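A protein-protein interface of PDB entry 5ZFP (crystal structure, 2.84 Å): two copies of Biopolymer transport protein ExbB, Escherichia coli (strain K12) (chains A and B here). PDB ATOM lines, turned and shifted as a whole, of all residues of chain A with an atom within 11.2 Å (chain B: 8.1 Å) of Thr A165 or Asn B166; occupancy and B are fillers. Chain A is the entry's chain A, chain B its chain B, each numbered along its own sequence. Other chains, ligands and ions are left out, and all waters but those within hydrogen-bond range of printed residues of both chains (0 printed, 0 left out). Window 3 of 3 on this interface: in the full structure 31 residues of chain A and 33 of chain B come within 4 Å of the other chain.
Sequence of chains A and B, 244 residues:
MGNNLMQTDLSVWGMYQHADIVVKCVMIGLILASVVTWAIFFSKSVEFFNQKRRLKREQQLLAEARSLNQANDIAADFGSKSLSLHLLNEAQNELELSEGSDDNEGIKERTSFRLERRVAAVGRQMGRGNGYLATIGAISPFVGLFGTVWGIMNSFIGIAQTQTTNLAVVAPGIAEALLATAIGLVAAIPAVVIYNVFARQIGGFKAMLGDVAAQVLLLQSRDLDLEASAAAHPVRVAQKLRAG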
ATOM      1  N   ASN A 154      -2.494 -29.557  30.075  1.00  0.00           N
ATOM      2  CA  ASN A 154      -2.540 -28.161  29.642  1.00  0.00           C
ATOM      3  C   ASN A 154      -2.006 -27.969  28.210  1.00  0.00           C
ATOM      4  O   ASN A 154      -2.479 -27.056  27.537  1.00  0.00           O
ATOM      5  CB  ASN A 154      -1.861 -27.234  30.650  1.00  0.00           C
ATOM      6  CG  ASN A 154      -2.726 -26.964  31.860  1.00  0.00           C
ATOM      7  OD1 ASN A 154      -3.772 -26.318  31.781  1.00  0.00           O
ATOM      8  ND2 ASN A 154      -2.321 -27.462  33.010  1.00  0.00           N
ATOM      9  N   SER A 155      -1.083 -28.847  27.717  1.00  0.00           N
ATOM     10  CA  SER A 155      -0.593 -28.818  26.320  1.00  0.00           C
ATOM     11  C   SER A 155      -1.741 -29.193  25.389  1.00  0.00           C
ATOM     12  O   SER A 155      -1.887 -28.578  24.340  1.00  0.00           O
ATOM     13  CB  SER A 155       0.562 -29.789  26.097  1.00  0.00           C
ATOM     14  OG  SER A 155       1.769 -29.339  26.679  1.00  0.00           O
ATOM     15  N   PHE A 156      -2.585 -30.164  25.788  1.00  0.00           N
ATOM     16  CA  PHE A 156      -3.760 -30.587  25.019  1.00  0.00           C
ATOM     17  C   PHE A 156      -4.861 -29.542  25.055  1.00  0.00           C
ATOM     18  O   PHE A 156      -5.553 -29.362  24.049  1.00  0.00           O
ATOM     19  CB  PHE A 156      -4.268 -31.963  25.455  1.00  0.00           C
ATOM     20  CG  PHE A 156      -3.462 -33.067  24.831  1.00  0.00           C
ATOM     21  CD1 PHE A 156      -3.697 -33.462  23.520  1.00  0.00           C
ATOM     22  CD2 PHE A 156      -2.438 -33.683  25.536  1.00  0.00           C
ATOM     23  CE1 PHE A 156      -2.939 -34.476  22.941  1.00  0.00           C
ATOM     24  CE2 PHE A 156      -1.688 -34.699  24.962  1.00  0.00           C
ATOM     25  CZ  PHE A 156      -1.937 -35.086  23.664  1.00  0.00           C
ATOM     26  N   ILE A 157      -4.990 -28.813  26.190  1.00  0.00           N
ATOM     27  CA  ILE A 157      -5.961 -27.720  26.320  1.00  0.00           C
ATOM     28  C   ILE A 157      -5.527 -26.613  25.341  1.00  0.00           C
ATOM     29  O   ILE A 157      -6.367 -26.039  24.663  1.00  0.00           O
ATOM     30  CB  ILE A 157      -6.126 -27.229  27.783  1.00  0.00           C
ATOM     31  CG1 ILE A 157      -6.804 -28.312  28.658  1.00  0.00           C
ATOM     32  CG2 ILE A 157      -6.898 -25.897  27.836  1.00  0.00           C
ATOM     33  CD1 ILE A 157      -6.612 -28.190  30.152  1.00  0.00           C
ATOM     34  N   GLY A 158      -4.219 -26.395  25.228  1.00  0.00           N
ATOM     35  CA  GLY A 158      -3.619 -25.454  24.289  1.00  0.00           C
ATOM     36  C   GLY A 158      -3.952 -25.773  22.838  1.00  0.00           C
ATOM     37  O   GLY A 158      -4.300 -24.863  22.084  1.00  0.00           O
ATOM     38  N   ILE A 159      -3.889 -27.080  22.440  1.00  0.00           N
ATOM     39  CA  ILE A 159      -4.229 -27.546  21.077  1.00  0.00           C
ATOM     40  C   ILE A 159      -5.717 -27.266  20.776  1.00  0.00           C
ATOM     41  O   ILE A 159      -6.055 -26.910  19.647  1.00  0.00           O
ATOM     42  CB  ILE A 159      -3.862 -29.048  20.841  1.00  0.00           C
ATOM     43  CG1 ILE A 159      -2.342 -29.256  20.805  1.00  0.00           C
ATOM     44  CG2 ILE A 159      -4.496 -29.597  19.550  1.00  0.00           C
ATOM     45  CD1 ILE A 159      -1.918 -30.702  20.892  1.00  0.00           C
ATOM     46  N   ALA A 160      -6.596 -27.460  21.785  1.00  0.00           N
ATOM     47  CA  ALA A 160      -8.042 -27.255  21.698  1.00  0.00           C
ATOM     48  C   ALA A 160      -8.425 -25.763  21.653  1.00  0.00           C
ATOM     49  O   ALA A 160      -9.180 -25.356  20.770  1.00  0.00           O
ATOM     50  CB  ALA A 160      -8.717 -27.933  22.878  1.00  0.00           C
ATOM     51  N   GLN A 161      -7.930 -24.965  22.626  1.00  0.00           N
ATOM     52  CA  GLN A 161      -8.184 -23.530  22.763  1.00  0.00           C
ATOM     53  C   GLN A 161      -7.733 -22.831  21.495  1.00  0.00           C
ATOM     54  O   GLN A 161      -8.586 -22.401  20.734  1.00  0.00           O
ATOM     55  CB  GLN A 161      -7.505 -22.954  24.027  1.00  0.00           C
ATOM     56  CG  GLN A 161      -8.015 -21.568  24.421  1.00  0.00           C
ATOM     57  CD  GLN A 161      -6.996 -20.742  25.170  1.00  0.00           C
ATOM     58  OE1 GLN A 161      -5.855 -21.158  25.416  1.00  0.00           O
ATOM     59  NE2 GLN A 161      -7.389 -19.531  25.538  1.00  0.00           N
ATOM     60  N   THR A 162      -6.418 -22.786  21.221  1.00  0.00           N
ATOM     61  CA  THR A 162      -5.886 -22.240  19.965  1.00  0.00           C
ATOM     62  C   THR A 162      -6.283 -23.258  18.872  1.00  0.00           C
ATOM     63  O   THR A 162      -6.130 -24.459  19.089  1.00  0.00           O
ATOM     64  CB  THR A 162      -4.341 -22.091  20.011  1.00  0.00           C
ATOM     65  OG1 THR A 162      -3.713 -23.293  19.568  1.00  0.00           O
ATOM     66  CG2 THR A 162      -3.807 -21.688  21.380  1.00  0.00           C
ATOM     67  N   GLN A 163      -6.798 -22.814  17.729  1.00  0.00           N
ATOM     68  CA  GLN A 163      -7.192 -23.754  16.678  1.00  0.00           C
ATOM     69  C   GLN A 163      -6.053 -24.694  16.235  1.00  0.00           C
ATOM     70  O   GLN A 163      -6.280 -25.883  16.030  1.00  0.00           O
ATOM     71  CB  GLN A 163      -7.765 -22.994  15.468  1.00  0.00           C
ATOM     72  CG  GLN A 163      -9.255 -22.660  15.617  1.00  0.00           C
ATOM     73  CD  GLN A 163      -9.645 -21.331  15.010  1.00  0.00           C
ATOM     74  OE1 GLN A 163      -9.052 -20.857  14.028  1.00  0.00           O
ATOM     75  NE2 GLN A 163     -10.666 -20.700  15.584  1.00  0.00           N
ATOM     76  N   THR A 164      -4.827 -24.150  16.148  1.00  0.00           N
ATOM     77  CA  THR A 164      -3.603 -24.793  15.672  1.00  0.00           C
ATOM     78  C   THR A 164      -2.983 -25.839  16.626  1.00  0.00           C
ATOM     79  O   THR A 164      -3.271 -25.868  17.817  1.00  0.00           O
ATOM     80  CB  THR A 164      -2.586 -23.702  15.280  1.00  0.00           C
ATOM     81  OG1 THR A 164      -1.365 -24.295  14.831  1.00  0.00           O
ATOM     82  CG2 THR A 164      -2.328 -22.685  16.390  1.00  0.00           C
ATOM     83  N   THR A 165      -2.129 -26.701  16.045  1.00  0.00           N
ATOM     84  CA  THR A 165      -1.349 -27.769  16.677  1.00  0.00           C
ATOM     85  C   THR A 165       0.110 -27.695  16.140  1.00  0.00           C
ATOM     86  O   THR A 165       0.393 -28.138  15.026  1.00  0.00           O
ATOM     87  CB  THR A 165      -2.065 -29.168  16.582  1.00  0.00           C
ATOM     88  OG1 THR A 165      -1.154 -30.228  16.889  1.00  0.00           O
ATOM     89  CG2 THR A 165      -2.732 -29.438  15.225  1.00  0.00           C
ATOM     90  N   ASN A 166       1.006 -27.043  16.915  1.00  0.00           N
ATOM     91  CA  ASN A 166       2.435 -26.857  16.601  1.00  0.00           C
ATOM     92  C   ASN A 166       3.319 -26.795  17.880  1.00  0.00           C
ATOM     93  O   ASN A 166       2.785 -26.789  18.994  1.00  0.00           O
ATOM     94  CB  ASN A 166       2.662 -25.628  15.679  1.00  0.00           C
ATOM     95  CG  ASN A 166       2.255 -24.273  16.236  1.00  0.00           C
ATOM     96  OD1 ASN A 166       1.544 -23.505  15.586  1.00  0.00           O
ATOM     97  ND2 ASN A 166       2.775 -23.890  17.386  1.00  0.00           N
ATOM     98  N   LEU A 167       4.656 -26.718  17.714  1.00  0.00           N
ATOM     99  CA  LEU A 167       5.611 -26.678  18.828  1.00  0.00           C
ATOM    100  C   LEU A 167       5.339 -25.570  19.834  1.00  0.00           C
ATOM    101  O   LEU A 167       5.411 -25.823  21.036  1.00  0.00           O
ATOM    102  CB  LEU A 167       7.080 -26.586  18.348  1.00  0.00           C
ATOM    103  CG  LEU A 167       7.826 -27.875  18.036  1.00  0.00           C
ATOM    104  CD1 LEU A 167       9.247 -27.566  17.699  1.00  0.00           C
ATOM    105  CD2 LEU A 167       7.772 -28.876  19.192  1.00  0.00           C
ATOM    106  N   ALA A 168       5.028 -24.353  19.344  1.00  0.00           N
ATOM    107  CA  ALA A 168       4.769 -23.183  20.180  1.00  0.00           C
ATOM    108  C   ALA A 168       3.528 -23.307  21.033  1.00  0.00           C
ATOM    109  O   ALA A 168       3.539 -22.826  22.167  1.00  0.00           O
ATOM    110  CB  ALA A 168       4.709 -21.925  19.333  1.00  0.00           C
ATOM    111  N   VAL A 169       2.462 -23.934  20.511  1.00  0.00           N
ATOM    112  CA  VAL A 169       1.183 -24.113  21.236  1.00  0.00           C
ATOM    113  C   VAL A 169       1.331 -25.036  22.448  1.00  0.00           C
ATOM    114  O   VAL A 169       0.798 -24.731  23.514  1.00  0.00           O
ATOM    115  CB  VAL A 169       0.047 -24.577  20.286  1.00  0.00           C
ATOM    116  CG1 VAL A 169      -1.193 -24.986  21.058  1.00  0.00           C
ATOM    117  CG2 VAL A 169      -0.286 -23.497  19.271  1.00  0.00           C
ATOM    118  N   VAL A 170       2.058 -26.151  22.275  1.00  0.00           N
ATOM    119  CA  VAL A 170       2.284 -27.175  23.300  1.00  0.00           C
ATOM    120  C   VAL A 170       3.467 -26.867  24.238  1.00  0.00           C
ATOM    121  O   VAL A 170       3.527 -27.462  25.317  1.00  0.00           O
ATOM    122  CB  VAL A 170       2.395 -28.615  22.710  1.00  0.00           C
ATOM    123  CG1 VAL A 170       1.063 -29.097  22.165  1.00  0.00           C
ATOM    124  CG2 VAL A 170       3.486 -28.730  21.654  1.00  0.00           C
ATOM    125  N   ALA A 171       4.393 -25.960  23.842  1.00  0.00           N
ATOM    126  CA  ALA A 171       5.575 -25.612  24.643  1.00  0.00           C
ATOM    127  C   ALA A 171       5.265 -25.206  26.084  1.00  0.00           C
ATOM    128  O   ALA A 171       5.913 -25.778  26.949  1.00  0.00           O
ATOM    129  CB  ALA A 171       6.425 -24.541  23.954  1.00  0.00           C
ATOM    130  N   PRO A 172       4.295 -24.301  26.418  1.00  0.00           N
ATOM    131  CA  PRO A 172       4.069 -23.965  27.840  1.00  0.00           C
ATOM    132  C   PRO A 172       3.663 -25.151  28.729  1.00  0.00           C
ATOM    133  O   PRO A 172       4.113 -25.232  29.867  1.00  0.00           O
ATOM    134  CB  PRO A 172       2.975 -22.891  27.777  1.00  0.00           C
ATOM    135  CG  PRO A 172       3.077 -22.327  26.424  1.00  0.00           C
ATOM    136  CD  PRO A 172       3.396 -23.502  25.562  1.00  0.00           C
ATOM    137  N   ILE A 174       4.393 -28.458  28.092  1.00  0.00           N
ATOM    138  CA  ILE A 174       5.555 -29.356  28.119  1.00  0.00           C
ATOM    139  C   ILE A 174       6.618 -28.847  29.103  1.00  0.00           C
ATOM    140  O   ILE A 174       7.141 -29.650  29.880  1.00  0.00           O
ATOM    141  CB  ILE A 174       6.120 -29.647  26.703  1.00  0.00           C
ATOM    142  CG1 ILE A 174       5.125 -30.485  25.873  1.00  0.00           C
ATOM    143  CG2 ILE A 174       7.488 -30.332  26.754  1.00  0.00           C
ATOM    144  CD1 ILE A 174       5.410 -30.484  24.337  1.00  0.00           C
ATOM    145  N   ILE B 159     -12.322 -40.855  16.162  1.00  0.00           N
ATOM    146  CA  ILE B 159     -11.500 -40.606  14.968  1.00  0.00           C
ATOM    147  C   ILE B 159     -11.803 -41.660  13.891  1.00  0.00           C
ATOM    148  O   ILE B 159     -12.012 -41.300  12.742  1.00  0.00           O
ATOM    149  CB  ILE B 159      -9.987 -40.454  15.295  1.00  0.00           C
ATOM    150  CG1 ILE B 159      -9.751 -39.203  16.170  1.00  0.00           C
ATOM    151  CG2 ILE B 159      -9.135 -40.391  14.028  1.00  0.00           C
ATOM    152  CD1 ILE B 159      -8.422 -39.133  16.882  1.00  0.00           C
ATOM    153  N   GLN B 163     -13.368 -40.248  10.617  1.00  0.00           N
ATOM    154  CA  GLN B 163     -12.175 -40.102   9.753  1.00  0.00           C
ATOM    155  C   GLN B 163     -11.471 -38.725   9.934  1.00  0.00           C
ATOM    156  O   GLN B 163     -10.910 -38.204   8.963  1.00  0.00           O
ATOM    157  CB  GLN B 163     -12.439 -40.424   8.261  1.00  0.00           C
ATOM    158  CG  GLN B 163     -13.032 -41.799   7.998  1.00  0.00           C
ATOM    159  CD  GLN B 163     -11.997 -42.882   7.981  1.00  0.00           C
ATOM    160  OE1 GLN B 163     -11.549 -43.367   9.028  1.00  0.00           O
ATOM    161  NE2 GLN B 163     -11.633 -43.316   6.788  1.00  0.00           N
ATOM    162  N   THR B 164     -11.461 -38.160  11.179  1.00  0.00           N
ATOM    163  CA  THR B 164     -10.768 -36.886  11.462  1.00  0.00           C
ATOM    164  C   THR B 164      -9.252 -37.036  11.387  1.00  0.00           C
ATOM    165  O   THR B 164      -8.709 -38.111  11.646  1.00  0.00           O
ATOM    166  CB  THR B 164     -11.204 -36.191  12.774  1.00  0.00           C
ATOM    167  OG1 THR B 164     -11.155 -37.102  13.864  1.00  0.00           O
ATOM    168  CG2 THR B 164     -12.572 -35.547  12.682  1.00  0.00           C
ATOM    169  N   THR B 165      -8.580 -35.952  10.993  1.00  0.00           N
ATOM    170  CA  THR B 165      -7.129 -35.883  10.830  1.00  0.00           C
ATOM    171  C   THR B 165      -6.553 -34.724  11.662  1.00  0.00           C
ATOM    172  O   THR B 165      -5.335 -34.607  11.789  1.00  0.00           O
ATOM    173  CB  THR B 165      -6.773 -35.757   9.338  1.00  0.00           C
ATOM    174  OG1 THR B 165      -7.257 -34.507   8.855  1.00  0.00           O
ATOM    175  CG2 THR B 165      -7.312 -36.914   8.480  1.00  0.00           C
ATOM    176  N   ASN B 166      -7.437 -33.879  12.236  1.00  0.00           N
ATOM    177  CA  ASN B 166      -7.072 -32.729  13.066  1.00  0.00           C
ATOM    178  C   ASN B 166      -7.090 -33.077  14.573  1.00  0.00           C
ATOM    179  O   ASN B 166      -8.155 -33.353  15.134  1.00  0.00           O
ATOM    180  CB  ASN B 166      -7.990 -31.539  12.764  1.00  0.00           C
ATOM    181  CG  ASN B 166      -7.471 -30.179  13.189  1.00  0.00           C
ATOM    182  OD1 ASN B 166      -8.025 -29.147  12.788  1.00  0.00           O
ATOM    183  ND2 ASN B 166      -6.403 -30.116  13.997  1.00  0.00           N
ATOM    184  N   LEU B 167      -5.908 -33.024  15.226  1.00  0.00           N
ATOM    185  CA  LEU B 167      -5.744 -33.302  16.656  1.00  0.00           C
ATOM    186  C   LEU B 167      -6.580 -32.352  17.537  1.00  0.00           C
ATOM    187  O   LEU B 167      -6.992 -32.756  18.626  1.00  0.00           O
ATOM    188  CB  LEU B 167      -4.241 -33.235  17.031  1.00  0.00           C
ATOM    189  CG  LEU B 167      -3.760 -33.784  18.397  1.00  0.00           C
ATOM    190  CD1 LEU B 167      -4.045 -35.282  18.568  1.00  0.00           C
ATOM    191  CD2 LEU B 167      -2.291 -33.554  18.554  1.00  0.00           C
ATOM    192  N   ALA B 168      -6.839 -31.109  17.055  1.00  0.00           N
ATOM    193  CA  ALA B 168      -7.603 -30.083  17.767  1.00  0.00           C
ATOM    194  C   ALA B 168      -9.031 -30.503  18.115  1.00  0.00           C
ATOM    195  O   ALA B 168      -9.524 -30.151  19.192  1.00  0.00           O
ATOM    196  CB  ALA B 168      -7.612 -28.792  16.976  1.00  0.00           C
ATOM    197  N   VAL B 169      -9.692 -31.262  17.222  1.00  0.00           N
ATOM    198  CA  VAL B 169     -11.065 -31.710  17.469  1.00  0.00           C
ATOM    199  C   VAL B 169     -11.133 -32.795  18.576  1.00  0.00           C
ATOM    200  O   VAL B 169     -12.176 -32.966  19.210  1.00  0.00           O
ATOM    201  CB  VAL B 169     -11.829 -32.127  16.174  1.00  0.00           C
ATOM    202  CG1 VAL B 169     -12.026 -30.936  15.242  1.00  0.00           C
ATOM    203  CG2 VAL B 169     -11.159 -33.287  15.444  1.00  0.00           C
ATOM    204  N   VAL B 170     -10.013 -33.477  18.832  1.00  0.00           N
ATOM    205  CA  VAL B 170      -9.938 -34.566  19.791  1.00  0.00           C
ATOM    206  C   VAL B 170      -9.089 -34.225  21.078  1.00  0.00           C
ATOM    207  O   VAL B 170      -9.018 -35.043  21.990  1.00  0.00           O
ATOM    208  CB  VAL B 170      -9.470 -35.824  19.021  1.00  0.00           C
ATOM    209  CG1 VAL B 170      -7.948 -35.992  19.004  1.00  0.00           C
ATOM    210  CG2 VAL B 170     -10.181 -37.067  19.513  1.00  0.00           C
ATOM    211  N   ALA B 171      -8.514 -33.012  21.162  1.00  0.00           N
ATOM    212  CA  ALA B 171      -7.766 -32.471  22.304  1.00  0.00           C
ATOM    213  C   ALA B 171      -8.632 -32.264  23.600  1.00  0.00           C
ATOM    214  O   ALA B 171      -8.150 -32.632  24.682  1.00  0.00           O
ATOM    215  CB  ALA B 171      -7.069 -31.183  21.905  1.00  0.00           C
ATOM    216  N   PRO B 172      -9.897 -31.739  23.551  1.00  0.00           N
ATOM    217  CA  PRO B 172     -10.677 -31.604  24.795  1.00  0.00           C
ATOM    218  C   PRO B 172     -10.961 -32.935  25.518  1.00  0.00           C
ATOM    219  O   PRO B 172     -10.958 -32.968  26.748  1.00  0.00           O
ATOM    220  CB  PRO B 172     -11.969 -30.912  24.328  1.00  0.00           C
ATOM    221  CG  PRO B 172     -11.626 -30.264  23.046  1.00  0.00           C
ATOM    222  CD  PRO B 172     -10.671 -31.212  22.404  1.00  0.00           C
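Among the printed residues, pairs that only touch across the chains: Phe A156 with Ala B171 (3.2 Å), Gln A163 with Ala B168 (3.3 Å), Ile A159 with Ala B168 (3.6 Å), Ile A159 with Leu B167 (3.7 Å), Ala A160 with Pro B172 (3.7 Å), Ala A160 with Ala B171 (3.8 Å), Ile A159 with Ala B171 (3.8 Å), Thr A165 with Leu B167 (3.9 Å) and Thr A165 with Asn B166 (3.9 Å).
Thr A165 touches just these residues of chain B: Asn B166 (3.9 Å) and Leu B167 (3.9 Å).
Asn B166 touches one residue of chain A.
No residue of chain B comes within 4 Å of Thr A164.
No residue of chain A comes within 4 Å of Thr B164.
Leu B167 touches just these residues of chain A: Ile A159 (3.7 Å) and Thr A165 (3.9 Å).
Ala B168 touches just these residues of chain A: Ile A159 (3.6 Å) and Gln A163 (3.3 Å).
Printed residues of chain B within 4 Å of Phe A156: Ala B171.
Of the printed residues of chain A, Pro B172 touches Ala A160.
Of the printed residues of chain B, Gln A163 touches Ala B168 (3.3 Å).
Of the printed residues of chain B, Ile A159 touches Leu B167 (3.7 Å), Ala B168 (3.6 Å) and Ala B171 (3.8 Å).
Of the printed residues of chain B, Ala A160 touches Ala B171 and Pro B172.
Ile A157 touches none of the printed residues of chain B.
Val A169 touches none of the printed residues of chain B.
Ile A159 touches Leu B167, but with the chains exchanged Leu A167 does not touch Ile B159 (18.1 Å).
Ile A159 touches Ala B168, but with the chains exchanged Ala A168 does not touch Ile B159 (20.1 Å).
Gln A163 touches Ala B168, but with the chains exchanged Ala A168 does not touch Gln B163 (23.5 Å).
Thr A165 touches Asn B166, but with the chains exchanged Asn A166 does not touch Thr B165 (11.1 Å).
11 positions are printed for both chains.
Of the 9 pairs that touch across the chains among the printed residues, none has its exchanged pair printed and touching as well.
The backbone NH (N) of Ala B168 lies close to the side-chain amide nitrogen (ND2) of Asn B166.
Of the 11 printed residues of chain B, 5 touch a printed residue of chain A.
Of the 20 printed residues of chain A, 5 touch a printed residue of chain B.
Hydrophobic or aromatic side chains of chain A that line the printed part of chain B: Ile A159 and Ala A160.
Among the printed residues, 9 pairs touch across the chains.
Among the printed residues, no Asp or Glu carboxylate lies within 4 Å of a Lys or Arg side-chain nitrogen of the other chain.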
